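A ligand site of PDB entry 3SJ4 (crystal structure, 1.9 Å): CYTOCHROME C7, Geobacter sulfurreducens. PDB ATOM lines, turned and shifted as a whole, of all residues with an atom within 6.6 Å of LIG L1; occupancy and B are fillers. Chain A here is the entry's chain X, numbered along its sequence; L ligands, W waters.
C25 of LIG L1 is bonded to SG of Cys 30, at 2.0 Å.
FE1 of LIG L1 is bound by NE2 of His 31 (2.0 Å).
A carbon (C18) of LIG L1 is covalently linked to the side-chain sulfur (SG) of Cys 27, 2.0 Å away.
FE1 of LIG L1 is bound by NE2 of His 17, 2.0 Å away.
N of Ala 1 sits at hydrogen-bond distance from O2 of LIG L1.
A ring nitrogen (NE2) of His 20 binds an iron atom (FE1) of LG2 L2 (2.1 Å).
The backbone NH of His 17 is in hydrogen-bond range of the side-chain carboxylate of Asp 3 (3.0 Å).
N of Phe 15 is in hydrogen-bond range of O of Ile 4 (3.0 Å).
The backbone carbonyl oxygen (O) of Pro 16 is in hydrogen-bond range of a ring nitrogen (ND1) of His 20 (2.7 Å).
The backbone carbonyl oxygen of Asp 2 lies close to an oxygen (O3) of LIG L1, at 3.4 Å.
CA of Asp 3 touches O4 of LIG L1, 3.6 Å away.
Ile 4 touches LIG L1 (CG2 to C33, 3.4 Å).
Phe 15 touches LIG L1.
His 20 touches LIG L1 (CD2 to C26, 3.8 Å).
Gln 21 touches LIG L1 (OE1 to C14, 3.4 Å).
Val 24 touches LIG L1.
Pro 25 touches LIG L1.
13 residues have an atom within 4 Å of LIG L1: Ala 1, Asp 2, Asp 3, Ile 4, Phe 15, His 17, His 20, Gln 21, Val 24, Pro 25, Cys 27, Cys 30 and His 31.
Water W3 lies within hydrogen-bond range of an oxygen (O3) of LIG L1 (2.7 Å), the backbone carbonyl oxygen (O) of Ala 1 (3.1 Å) and the side-chain carboxylate (OD1) of Asp 3 (3.1 Å).
Water W2 bridges ND1 of His 17 and O2 of LIG L1.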
ATOM      1  N   ALA A   1      33.963  17.640 -13.848  1.00  0.00           N
ATOM      2  CA  ALA A   1      32.913  18.652 -13.494  1.00  0.00           C
ATOM      3  C   ALA A   1      31.618  17.955 -13.149  1.00  0.00           C
ATOM      4  O   ALA A   1      31.394  16.809 -13.498  1.00  0.00           O
ATOM      5  CB  ALA A   1      32.681  19.624 -14.629  1.00  0.00           C
ATOM      6  N   ASP A   2      30.752  18.686 -12.490  1.00  0.00           N
ATOM      7  CA  ASP A   2      29.495  18.175 -12.053  1.00  0.00           C
ATOM      8  C   ASP A   2      28.439  18.426 -13.110  1.00  0.00           C
ATOM      9  O   ASP A   2      28.560  19.342 -13.906  1.00  0.00           O
ATOM     10  CB  ASP A   2      29.099  18.895 -10.785  1.00  0.00           C
ATOM     11  CG  ASP A   2      30.013  18.569  -9.666  1.00  0.00           C
ATOM     12  OD1 ASP A   2      30.141  17.347  -9.369  1.00  0.00           O
ATOM     13  OD2 ASP A   2      30.667  19.454  -9.066  1.00  0.00           O
ATOM     14  N   ASP A   3      27.388  17.607 -13.075  1.00  0.00           N
ATOM     15  CA  ASP A   3      26.197  17.864 -13.855  1.00  0.00           C
ATOM     16  C   ASP A   3      25.512  19.136 -13.385  1.00  0.00           C
ATOM     17  O   ASP A   3      25.786  19.639 -12.285  1.00  0.00           O
ATOM     18  CB  ASP A   3      25.200  16.714 -13.751  1.00  0.00           C
ATOM     19  CG  ASP A   3      25.683  15.467 -14.471  1.00  0.00           C
ATOM     20  OD1 ASP A   3      26.560  15.577 -15.352  1.00  0.00           O
ATOM     21  OD2 ASP A   3      25.216  14.359 -14.220  1.00  0.00           O
ATOM     22  N   ILE A   4      24.643  19.665 -14.228  1.00  0.00           N
ATOM     23  CA  ILE A   4      23.936  20.866 -13.850  1.00  0.00           C
ATOM     24  C   ILE A   4      22.446  20.615 -13.879  1.00  0.00           C
ATOM     25  O   ILE A   4      21.980  19.697 -14.541  1.00  0.00           O
ATOM     26  CB  ILE A   4      24.325  22.061 -14.777  1.00  0.00           C
ATOM     27  CG1 ILE A   4      23.460  22.149 -16.034  1.00  0.00           C
ATOM     28  CG2 ILE A   4      25.779  21.968 -15.246  1.00  0.00           C
ATOM     29  CD1 ILE A   4      22.196  22.996 -15.871  1.00  0.00           C
ATOM     30  N   PHE A  15      20.603  17.667 -16.324  1.00  0.00           N
ATOM     31  CA  PHE A  15      21.332  17.428 -17.552  1.00  0.00           C
ATOM     32  C   PHE A  15      22.498  16.507 -17.205  1.00  0.00           C
ATOM     33  O   PHE A  15      23.470  16.951 -16.582  1.00  0.00           O
ATOM     34  CB  PHE A  15      21.859  18.722 -18.188  1.00  0.00           C
ATOM     35  CG  PHE A  15      22.700  18.461 -19.387  1.00  0.00           C
ATOM     36  CD1 PHE A  15      22.122  18.038 -20.574  1.00  0.00           C
ATOM     37  CD2 PHE A  15      24.083  18.521 -19.298  1.00  0.00           C
ATOM     38  CE1 PHE A  15      22.885  17.739 -21.679  1.00  0.00           C
ATOM     39  CE2 PHE A  15      24.864  18.199 -20.411  1.00  0.00           C
ATOM     40  CZ  PHE A  15      24.259  17.813 -21.590  1.00  0.00           C
ATOM     41  N   PRO A  16      22.371  15.210 -17.485  1.00  0.00           N
ATOM     42  CA  PRO A  16      23.439  14.238 -17.209  1.00  0.00           C
ATOM     43  C   PRO A  16      24.436  14.165 -18.347  1.00  0.00           C
ATOM     44  O   PRO A  16      24.145  13.644 -19.430  1.00  0.00           O
ATOM     45  CB  PRO A  16      22.666  12.925 -17.028  1.00  0.00           C
ATOM     46  CG  PRO A  16      21.491  13.081 -17.943  1.00  0.00           C
ATOM     47  CD  PRO A  16      21.148  14.556 -17.998  1.00  0.00           C
ATOM     48  N   HIS A  17      25.638  14.696 -18.111  1.00  0.00           N
ATOM     49  CA  HIS A  17      26.619  14.772 -19.192  1.00  0.00           C
ATOM     50  C   HIS A  17      27.145  13.414 -19.653  1.00  0.00           C
ATOM     51  O   HIS A  17      27.307  13.190 -20.854  1.00  0.00           O
ATOM     52  CB  HIS A  17      27.800  15.656 -18.821  1.00  0.00           C
ATOM     53  CG  HIS A  17      28.750  15.886 -19.963  1.00  0.00           C
ATOM     54  ND1 HIS A  17      29.928  15.196 -20.094  1.00  0.00           N
ATOM     55  CD2 HIS A  17      28.678  16.715 -21.027  1.00  0.00           C
ATOM     56  CE1 HIS A  17      30.563  15.618 -21.169  1.00  0.00           C
ATOM     57  NE2 HIS A  17      29.829  16.551 -21.748  1.00  0.00           N
ATOM     58  N   LYS A  18      27.433  12.521 -18.728  1.00  0.00           N
ATOM     59  CA  LYS A  18      27.962  11.215 -19.117  1.00  0.00           C
ATOM     60  C   LYS A  18      27.089  10.531 -20.191  1.00  0.00           C
ATOM     61  O   LYS A  18      27.612  10.049 -21.195  1.00  0.00           O
ATOM     62  CB  LYS A  18      28.105  10.308 -17.877  1.00  0.00           C
ATOM     63  CG  LYS A  18      28.803   8.990 -18.159  1.00  0.00           C
ATOM     64  N   HIS A  20      25.187  11.822 -22.344  1.00  0.00           N
ATOM     65  CA  HIS A  20      25.259  12.588 -23.578  1.00  0.00           C
ATOM     66  C   HIS A  20      26.569  12.398 -24.359  1.00  0.00           C
ATOM     67  O   HIS A  20      26.559  12.288 -25.560  1.00  0.00           O
ATOM     68  CB  HIS A  20      24.993  14.051 -23.314  1.00  0.00           C
ATOM     69  CG  HIS A  20      23.556  14.323 -23.025  1.00  0.00           C
ATOM     70  ND1 HIS A  20      23.030  14.238 -21.762  1.00  0.00           N
ATOM     71  CD2 HIS A  20      22.513  14.603 -23.842  1.00  0.00           C
ATOM     72  CE1 HIS A  20      21.738  14.455 -21.811  1.00  0.00           C
ATOM     73  NE2 HIS A  20      21.396  14.686 -23.062  1.00  0.00           N
ATOM     74  N   GLN A  21      27.672  12.388 -23.634  1.00  0.00           N
ATOM     75  CA  GLN A  21      28.961  12.073 -24.222  1.00  0.00           C
ATOM     76  C   GLN A  21      28.919  10.703 -24.923  1.00  0.00           C
ATOM     77  O   GLN A  21      29.421  10.547 -26.020  1.00  0.00           O
ATOM     78  CB  GLN A  21      29.997  12.066 -23.105  1.00  0.00           C
ATOM     79  CG  GLN A  21      31.439  12.285 -23.531  1.00  0.00           C
ATOM     80  CD  GLN A  21      32.290  12.849 -22.371  1.00  0.00           C
ATOM     81  OE1 GLN A  21      33.223  13.623 -22.579  1.00  0.00           O
ATOM     82  NE2 GLN A  21      31.940  12.466 -21.161  1.00  0.00           N
ATOM     83  N   LYS A  22      28.291   9.722 -24.268  1.00  0.00           N
ATOM     84  CA  LYS A  22      28.168   8.367 -24.825  1.00  0.00           C
ATOM     85  C   LYS A  22      27.213   8.255 -26.033  1.00  0.00           C
ATOM     86  O   LYS A  22      27.543   7.642 -27.061  1.00  0.00           O
ATOM     87  CB  LYS A  22      27.744   7.405 -23.717  1.00  0.00           C
ATOM     88  CG  LYS A  22      27.716   5.954 -24.154  1.00  0.00           C
ATOM     89  N   VAL A  24      25.972  10.804 -27.903  1.00  0.00           N
ATOM     90  CA  VAL A  24      26.164  11.838 -28.898  1.00  0.00           C
ATOM     91  C   VAL A  24      27.665  12.041 -29.029  1.00  0.00           C
ATOM     92  O   VAL A  24      28.181  13.132 -28.709  1.00  0.00           O
ATOM     93  CB  VAL A  24      25.472  13.174 -28.531  1.00  0.00           C
ATOM     94  CG1 VAL A  24      25.502  14.121 -29.692  1.00  0.00           C
ATOM     95  CG2 VAL A  24      24.012  12.978 -28.097  1.00  0.00           C
ATOM     96  N   PRO A  25      28.341  10.986 -29.497  1.00  0.00           N
ATOM     97  CA  PRO A  25      29.809  11.034 -29.675  1.00  0.00           C
ATOM     98  C   PRO A  25      30.291  12.153 -30.592  1.00  0.00           C
ATOM     99  O   PRO A  25      31.463  12.538 -30.498  1.00  0.00           O
ATOM    100  CB  PRO A  25      30.139   9.642 -30.255  1.00  0.00           C
ATOM    101  CG  PRO A  25      28.824   9.141 -30.825  1.00  0.00           C
ATOM    102  CD  PRO A  25      27.791   9.670 -29.887  1.00  0.00           C
ATOM    103  N   ASP A  26      29.427  12.665 -31.448  1.00  0.00           N
ATOM    104  CA  ASP A  26      29.729  13.871 -32.183  1.00  0.00           C
ATOM    105  C   ASP A  26      29.622  15.120 -31.265  1.00  0.00           C
ATOM    106  O   ASP A  26      28.580  15.817 -31.202  1.00  0.00           O
ATOM    107  CB  ASP A  26      28.795  14.030 -33.373  1.00  0.00           C
ATOM    108  CG  ASP A  26      29.180  15.201 -34.241  1.00  0.00           C
ATOM    109  OD1 ASP A  26      30.184  15.876 -33.927  1.00  0.00           O
ATOM    110  OD2 ASP A  26      28.541  15.524 -35.249  1.00  0.00           O
ATOM    111  N   CYS A  27      30.726  15.417 -30.591  1.00  0.00           N
ATOM    112  CA  CYS A  27      30.768  16.487 -29.599  1.00  0.00           C
ATOM    113  C   CYS A  27      30.384  17.865 -30.143  1.00  0.00           C
ATOM    114  O   CYS A  27      29.878  18.700 -29.387  1.00  0.00           O
ATOM    115  CB  CYS A  27      32.134  16.557 -28.953  1.00  0.00           C
ATOM    116  SG  CYS A  27      32.923  14.951 -28.550  1.00  0.00           S
ATOM    117  N   LYS A  28      30.607  18.100 -31.432  1.00  0.00           N
ATOM    118  CA  LYS A  28      30.328  19.402 -32.032  1.00  0.00           C
ATOM    119  C   LYS A  28      28.834  19.705 -32.141  1.00  0.00           C
ATOM    120  O   LYS A  28      28.439  20.796 -32.567  1.00  0.00           O
ATOM    121  CB  LYS A  28      30.974  19.511 -33.422  1.00  0.00           C
ATOM    122  CG  LYS A  28      32.505  19.601 -33.401  1.00  0.00           C
ATOM    123  CD  LYS A  28      33.067  20.043 -34.753  1.00  0.00           C
ATOM    124  CE  LYS A  28      32.781  21.507 -35.028  1.00  0.00           C
ATOM    125  NZ  LYS A  28      33.317  21.931 -36.360  1.00  0.00           N
ATOM    126  N   LYS A  29      27.988  18.746 -31.785  1.00  0.00           N
ATOM    127  CA  LYS A  29      26.568  19.015 -31.615  1.00  0.00           C
ATOM    128  C   LYS A  29      26.347  20.034 -30.512  1.00  0.00           C
ATOM    129  O   LYS A  29      25.410  20.796 -30.595  1.00  0.00           O
ATOM    130  CB  LYS A  29      25.791  17.727 -31.316  1.00  0.00           C
ATOM    131  CG  LYS A  29      25.510  16.913 -32.552  1.00  0.00           C
ATOM    132  CD  LYS A  29      24.572  17.744 -33.468  1.00  0.00           C
ATOM    133  CE  LYS A  29      24.035  16.994 -34.666  1.00  0.00           C
ATOM    134  N   CYS A  30      27.212  20.058 -29.514  1.00  0.00           N
ATOM    135  CA  CYS A  30      27.098  21.011 -28.424  1.00  0.00           C
ATOM    136  C   CYS A  30      28.302  21.876 -28.146  1.00  0.00           C
ATOM    137  O   CYS A  30      28.155  22.966 -27.598  1.00  0.00           O
ATOM    138  CB  CYS A  30      26.811  20.246 -27.144  1.00  0.00           C
ATOM    139  SG  CYS A  30      25.229  19.348 -27.217  1.00  0.00           S
ATOM    140  N   HIS A  31      29.495  21.385 -28.469  1.00  0.00           N
ATOM    141  CA  HIS A  31      30.730  22.090 -28.160  1.00  0.00           C
ATOM    142  C   HIS A  31      31.342  22.816 -29.368  1.00  0.00           C
ATOM    143  O   HIS A  31      31.031  22.511 -30.522  1.00  0.00           O
ATOM    144  CB  HIS A  31      31.741  21.127 -27.527  1.00  0.00           C
ATOM    145  CG  HIS A  31      31.343  20.636 -26.180  1.00  0.00           C
ATOM    146  ND1 HIS A  31      31.031  21.489 -25.141  1.00  0.00           N
ATOM    147  CD2 HIS A  31      31.182  19.379 -25.692  1.00  0.00           C
ATOM    148  CE1 HIS A  31      30.714  20.774 -24.067  1.00  0.00           C
ATOM    149  NE2 HIS A  31      30.797  19.494 -24.380  1.00  0.00           N
ATOM    150  N   GLY A  50      17.570  22.638 -28.659  1.00  0.00           N
ATOM    151  CA  GLY A  50      18.398  22.637 -27.469  1.00  0.00           C
ATOM    152  C   GLY A  50      18.327  21.392 -26.588  1.00  0.00           C
ATOM    153  O   GLY A  50      19.347  20.978 -25.992  1.00  0.00           O
HETATM  154 FE1  LIG L   1      30.274  18.007 -23.120  1.00  0.00          FE
HETATM  155  C1  LIG L   1      30.930  19.523 -20.116  1.00  0.00           C
HETATM  156  C2  LIG L   1      33.523  17.166 -23.443  1.00  0.00           C
HETATM  157  C3  LIG L   1      29.461  15.904 -25.712  1.00  0.00           C
HETATM  158  C4  LIG L   1      27.217  19.443 -23.237  1.00  0.00           C
HETATM  159  N1  LIG L   1      31.900  18.355 -22.056  1.00  0.00           N
HETATM  160  C5  LIG L   1      31.950  18.854 -20.762  1.00  0.00           C
HETATM  161  C6  LIG L   1      33.245  18.611 -20.223  1.00  0.00           C
HETATM  162  C7  LIG L   1      33.977  17.970 -21.131  1.00  0.00           C
HETATM  163  C8  LIG L   1      33.144  17.807 -22.307  1.00  0.00           C
HETATM  164  C9  LIG L   1      35.433  17.508 -20.984  1.00  0.00           C
HETATM  165  C10 LIG L   1      33.697  18.934 -18.785  1.00  0.00           C
HETATM  166  C11 LIG L   1      33.331  17.588 -18.129  1.00  0.00           C
HETATM  167  C12 LIG L   1      33.911  17.378 -16.754  1.00  0.00           C
HETATM  168  O1  LIG L   1      34.997  17.956 -16.430  1.00  0.00           O
HETATM  169  O2  LIG L   1      33.275  16.595 -15.988  1.00  0.00           O
HETATM  170  N2  LIG L   1      31.298  16.728 -24.356  1.00  0.00           N
HETATM  171  C13 LIG L   1      32.661  16.538 -24.321  1.00  0.00           C
HETATM  172  C14 LIG L   1      33.015  15.580 -25.343  1.00  0.00           C
HETATM  173  C15 LIG L   1      31.875  15.225 -25.984  1.00  0.00           C
HETATM  174  C16 LIG L   1      30.788  15.947 -25.359  1.00  0.00           C
HETATM  175  C17 LIG L   1      34.472  15.092 -25.561  1.00  0.00           C
HETATM  176  C18 LIG L   1      31.647  14.224 -27.152  1.00  0.00           C
HETATM  177  C19 LIG L   1      32.200  12.981 -27.070  1.00  0.00           C
HETATM  178  N3  LIG L   1      28.685  17.711 -24.207  1.00  0.00           N
HETATM  179  C20 LIG L   1      28.526  16.812 -25.274  1.00  0.00           C
HETATM  180  C21 LIG L   1      27.214  16.988 -25.854  1.00  0.00           C
HETATM  181  C22 LIG L   1      26.583  17.947 -25.153  1.00  0.00           C
HETATM  182  C23 LIG L   1      27.494  18.434 -24.124  1.00  0.00           C
HETATM  183  C24 LIG L   1      26.719  16.169 -27.073  1.00  0.00           C
HETATM  184  C25 LIG L   1      25.185  18.538 -25.377  1.00  0.00           C
HETATM  185  C26 LIG L   1      24.090  17.697 -25.444  1.00  0.00           C
HETATM  186  N4  LIG L   1      29.240  19.328 -21.890  1.00  0.00           N
HETATM  187  C27 LIG L   1      27.977  19.780 -22.158  1.00  0.00           C
HETATM  188  C28 LIG L   1      27.583  20.654 -21.082  1.00  0.00           C
HETATM  189  C29 LIG L   1      28.726  20.678 -20.098  1.00  0.00           C
HETATM  190  C30 LIG L   1      29.713  19.825 -20.685  1.00  0.00           C
HETATM  191  C31 LIG L   1      26.263  21.395 -20.977  1.00  0.00           C
HETATM  192  C32 LIG L   1      28.806  21.440 -18.756  1.00  0.00           C
HETATM  193  C33 LIG L   1      27.807  20.816 -17.771  1.00  0.00           C
HETATM  194  C34 LIG L   1      28.095  19.381 -17.389  1.00  0.00           C
HETATM  195  O3  LIG L   1      29.270  18.996 -17.213  1.00  0.00           O
HETATM  196  O4  LIG L   1      27.121  18.614 -17.215  1.00  0.00           O
HETATM  197 FE1  LG2 L   2      19.506  14.647 -23.881  1.00  0.00          FE
HETATM  198  C1  LG2 L   2      19.347  11.407 -22.823  1.00  0.00           C
HETATM  199  C2  LG2 L   2      18.149  15.658 -20.889  1.00  0.00           C
HETATM  200  C3  LG2 L   2      20.061  17.901 -24.750  1.00  0.00           C
HETATM  201  C4  LG2 L   2      20.541  13.641 -26.968  1.00  0.00           C
HETATM  202  N1  LG2 L   2      18.854  13.719 -22.192  1.00  0.00           N
HETATM  203  C5  LG2 L   2      18.905  12.369 -21.949  1.00  0.00           C
HETATM  204  C6  LG2 L   2      18.451  12.125 -20.591  1.00  0.00           C
HETATM  205  C7  LG2 L   2      18.117  13.291 -20.052  1.00  0.00           C
HETATM  206  C8  LG2 L   2      18.378  14.317 -21.023  1.00  0.00           C
HETATM  207  C9  LG2 L   2      17.596  13.510 -18.621  1.00  0.00           C
HETATM  208  C10 LG2 L   2      18.343  10.729 -19.939  1.00  0.00           C
HETATM  209  C11 LG2 L   2      19.702  10.203 -19.549  1.00  0.00           C
HETATM  210  C12 LG2 L   2      19.640   8.762 -19.113  1.00  0.00           C
HETATM  211  O1  LG2 L   2      18.949   7.950 -19.779  1.00  0.00           O
HETATM  212  O2  LG2 L   2      20.293   8.428 -18.091  1.00  0.00           O
HETATM  213  N2  LG2 L   2      19.179  16.409 -22.987  1.00  0.00           N
HETATM  214  C13 LG2 L   2      18.559  16.631 -21.775  1.00  0.00           C
HETATM  215  C14 LG2 L   2      18.470  18.046 -21.542  1.00  0.00           C
HETATM  216  C15 LG2 L   2      19.018  18.680 -22.597  1.00  0.00           C
HETATM  217  C16 LG2 L   2      19.481  17.663 -23.527  1.00  0.00           C
HETATM  218  C17 LG2 L   2      17.814  18.626 -20.274  1.00  0.00           C
HETATM  219  C18 LG2 L   2      19.152  20.197 -22.814  1.00  0.00           C
HETATM  220  C19 LG2 L   2      19.588  20.976 -21.779  1.00  0.00           C
HETATM  221  N3  LG2 L   2      20.150  15.603 -25.536  1.00  0.00           N
HETATM  222  C20 LG2 L   2      20.306  16.961 -25.718  1.00  0.00           C
HETATM  223  C21 LG2 L   2      20.849  17.216 -27.030  1.00  0.00           C
HETATM  224  C22 LG2 L   2      20.990  16.024 -27.646  1.00  0.00           C
HETATM  225  C23 LG2 L   2      20.570  15.003 -26.716  1.00  0.00           C
HETATM  226  C24 LG2 L   2      21.154  18.625 -27.590  1.00  0.00           C
HETATM  227  C25 LG2 L   2      21.549  15.748 -29.077  1.00  0.00           C
HETATM  228  C26 LG2 L   2      22.175  16.733 -29.777  1.00  0.00           C
HETATM  229  N4  LG2 L   2      19.935  12.841 -24.745  1.00  0.00           N
HETATM  230  C27 LG2 L   2      20.258  12.657 -26.075  1.00  0.00           C
HETATM  231  C28 LG2 L   2      20.235  11.257 -26.403  1.00  0.00           C
HETATM  232  C29 LG2 L   2      19.873  10.560 -25.107  1.00  0.00           C
HETATM  233  C30 LG2 L   2      19.708  11.624 -24.138  1.00  0.00           C
HETATM  234  C31 LG2 L   2      20.519  10.579 -27.773  1.00  0.00           C
HETATM  235  C32 LG2 L   2      19.728   9.056 -24.828  1.00  0.00           C
HETATM  236  C33 LG2 L   2      20.838   8.668 -23.843  1.00  0.00           C
HETATM  237  C34 LG2 L   2      20.643   7.284 -23.271  1.00  0.00           C
HETATM  238  O3  LG2 L   2      19.478   6.854 -23.063  1.00  0.00           O
HETATM  239  O4  LG2 L   2      21.683   6.626 -23.008  1.00  0.00           O
HETATM  240  C1  LG3 L   3      22.287  27.834 -19.615  1.00  0.00           C
HETATM  241  C2  LG3 L   3      22.004  26.301 -19.778  1.00  0.00           C
HETATM  242  C3  LG3 L   3      23.318  25.480 -19.751  1.00  0.00           C
HETATM  243  C4  LG3 L   3      24.309  25.953 -20.837  1.00  0.00           C
HETATM  244  C5  LG3 L   3      24.575  27.461 -20.624  1.00  0.00           C
HETATM  245  C6  LG3 L   3      23.276  28.285 -20.703  1.00  0.00           C
HETATM  246  C7  LG3 L   3      22.985  23.969 -19.911  1.00  0.00           C
HETATM  247  C8  LG3 L   3      22.469  23.616 -21.314  1.00  0.00           C
HETATM  248  C9  LG3 L   3      23.478  24.081 -22.374  1.00  0.00           C
HETATM  249  C10 LG3 L   3      23.801  25.592 -22.249  1.00  0.00           C
HETATM  250  C11 LG3 L   3      23.022  23.747 -23.793  1.00  0.00           C
HETATM  251  C12 LG3 L   3      24.086  24.074 -24.887  1.00  0.00           C
HETATM  252  C13 LG3 L   3      24.385  25.569 -24.803  1.00  0.00           C
HETATM  253  C14 LG3 L   3      24.814  25.996 -23.388  1.00  0.00           C
HETATM  254  C15 LG3 L   3      22.661  22.259 -24.078  1.00  0.00           C
HETATM  255  C16 LG3 L   3      22.738  22.194 -25.620  1.00  0.00           C
HETATM  256  C17 LG3 L   3      23.291  23.562 -26.114  1.00  0.00           C
HETATM  257  C18 LG3 L   3      25.664  25.271 -20.602  1.00  0.00           C
HETATM  258  C19 LG3 L   3      24.058  23.390 -27.467  1.00  0.00           C
HETATM  259  O1  LG3 L   3      23.197  26.308 -25.119  1.00  0.00           O
HETATM  260  O2  LG3 L   3      21.052  28.583 -19.713  1.00  0.00           O
HETATM  261  C20 LG3 L   3      25.367  23.301 -24.669  1.00  0.00           C
HETATM  262  C21 LG3 L   3      23.233  22.655 -28.515  1.00  0.00           C
HETATM  263  C22 LG3 L   3      21.963  23.395 -28.858  1.00  0.00           C
HETATM  264  C23 LG3 L   3      22.110  24.302 -30.077  1.00  0.00           C
HETATM  265  O3  LG3 L   3      22.430  23.836 -31.164  1.00  0.00           O
HETATM  266  O4  LG3 L   3      21.902  25.512 -29.952  1.00  0.00           O
HETATM  267  C24 LG3 L   3      24.576  24.713 -28.069  1.00  0.00           C
HETATM  268  O   HOH W   1      36.083  13.829 -22.790  1.00  0.00           O
HETATM  269  O   HOH W   2      30.989  14.363 -17.353  1.00  0.00           O
HETATM  270  O   HOH W   3      29.465  16.614 -15.976  1.00  0.00           O
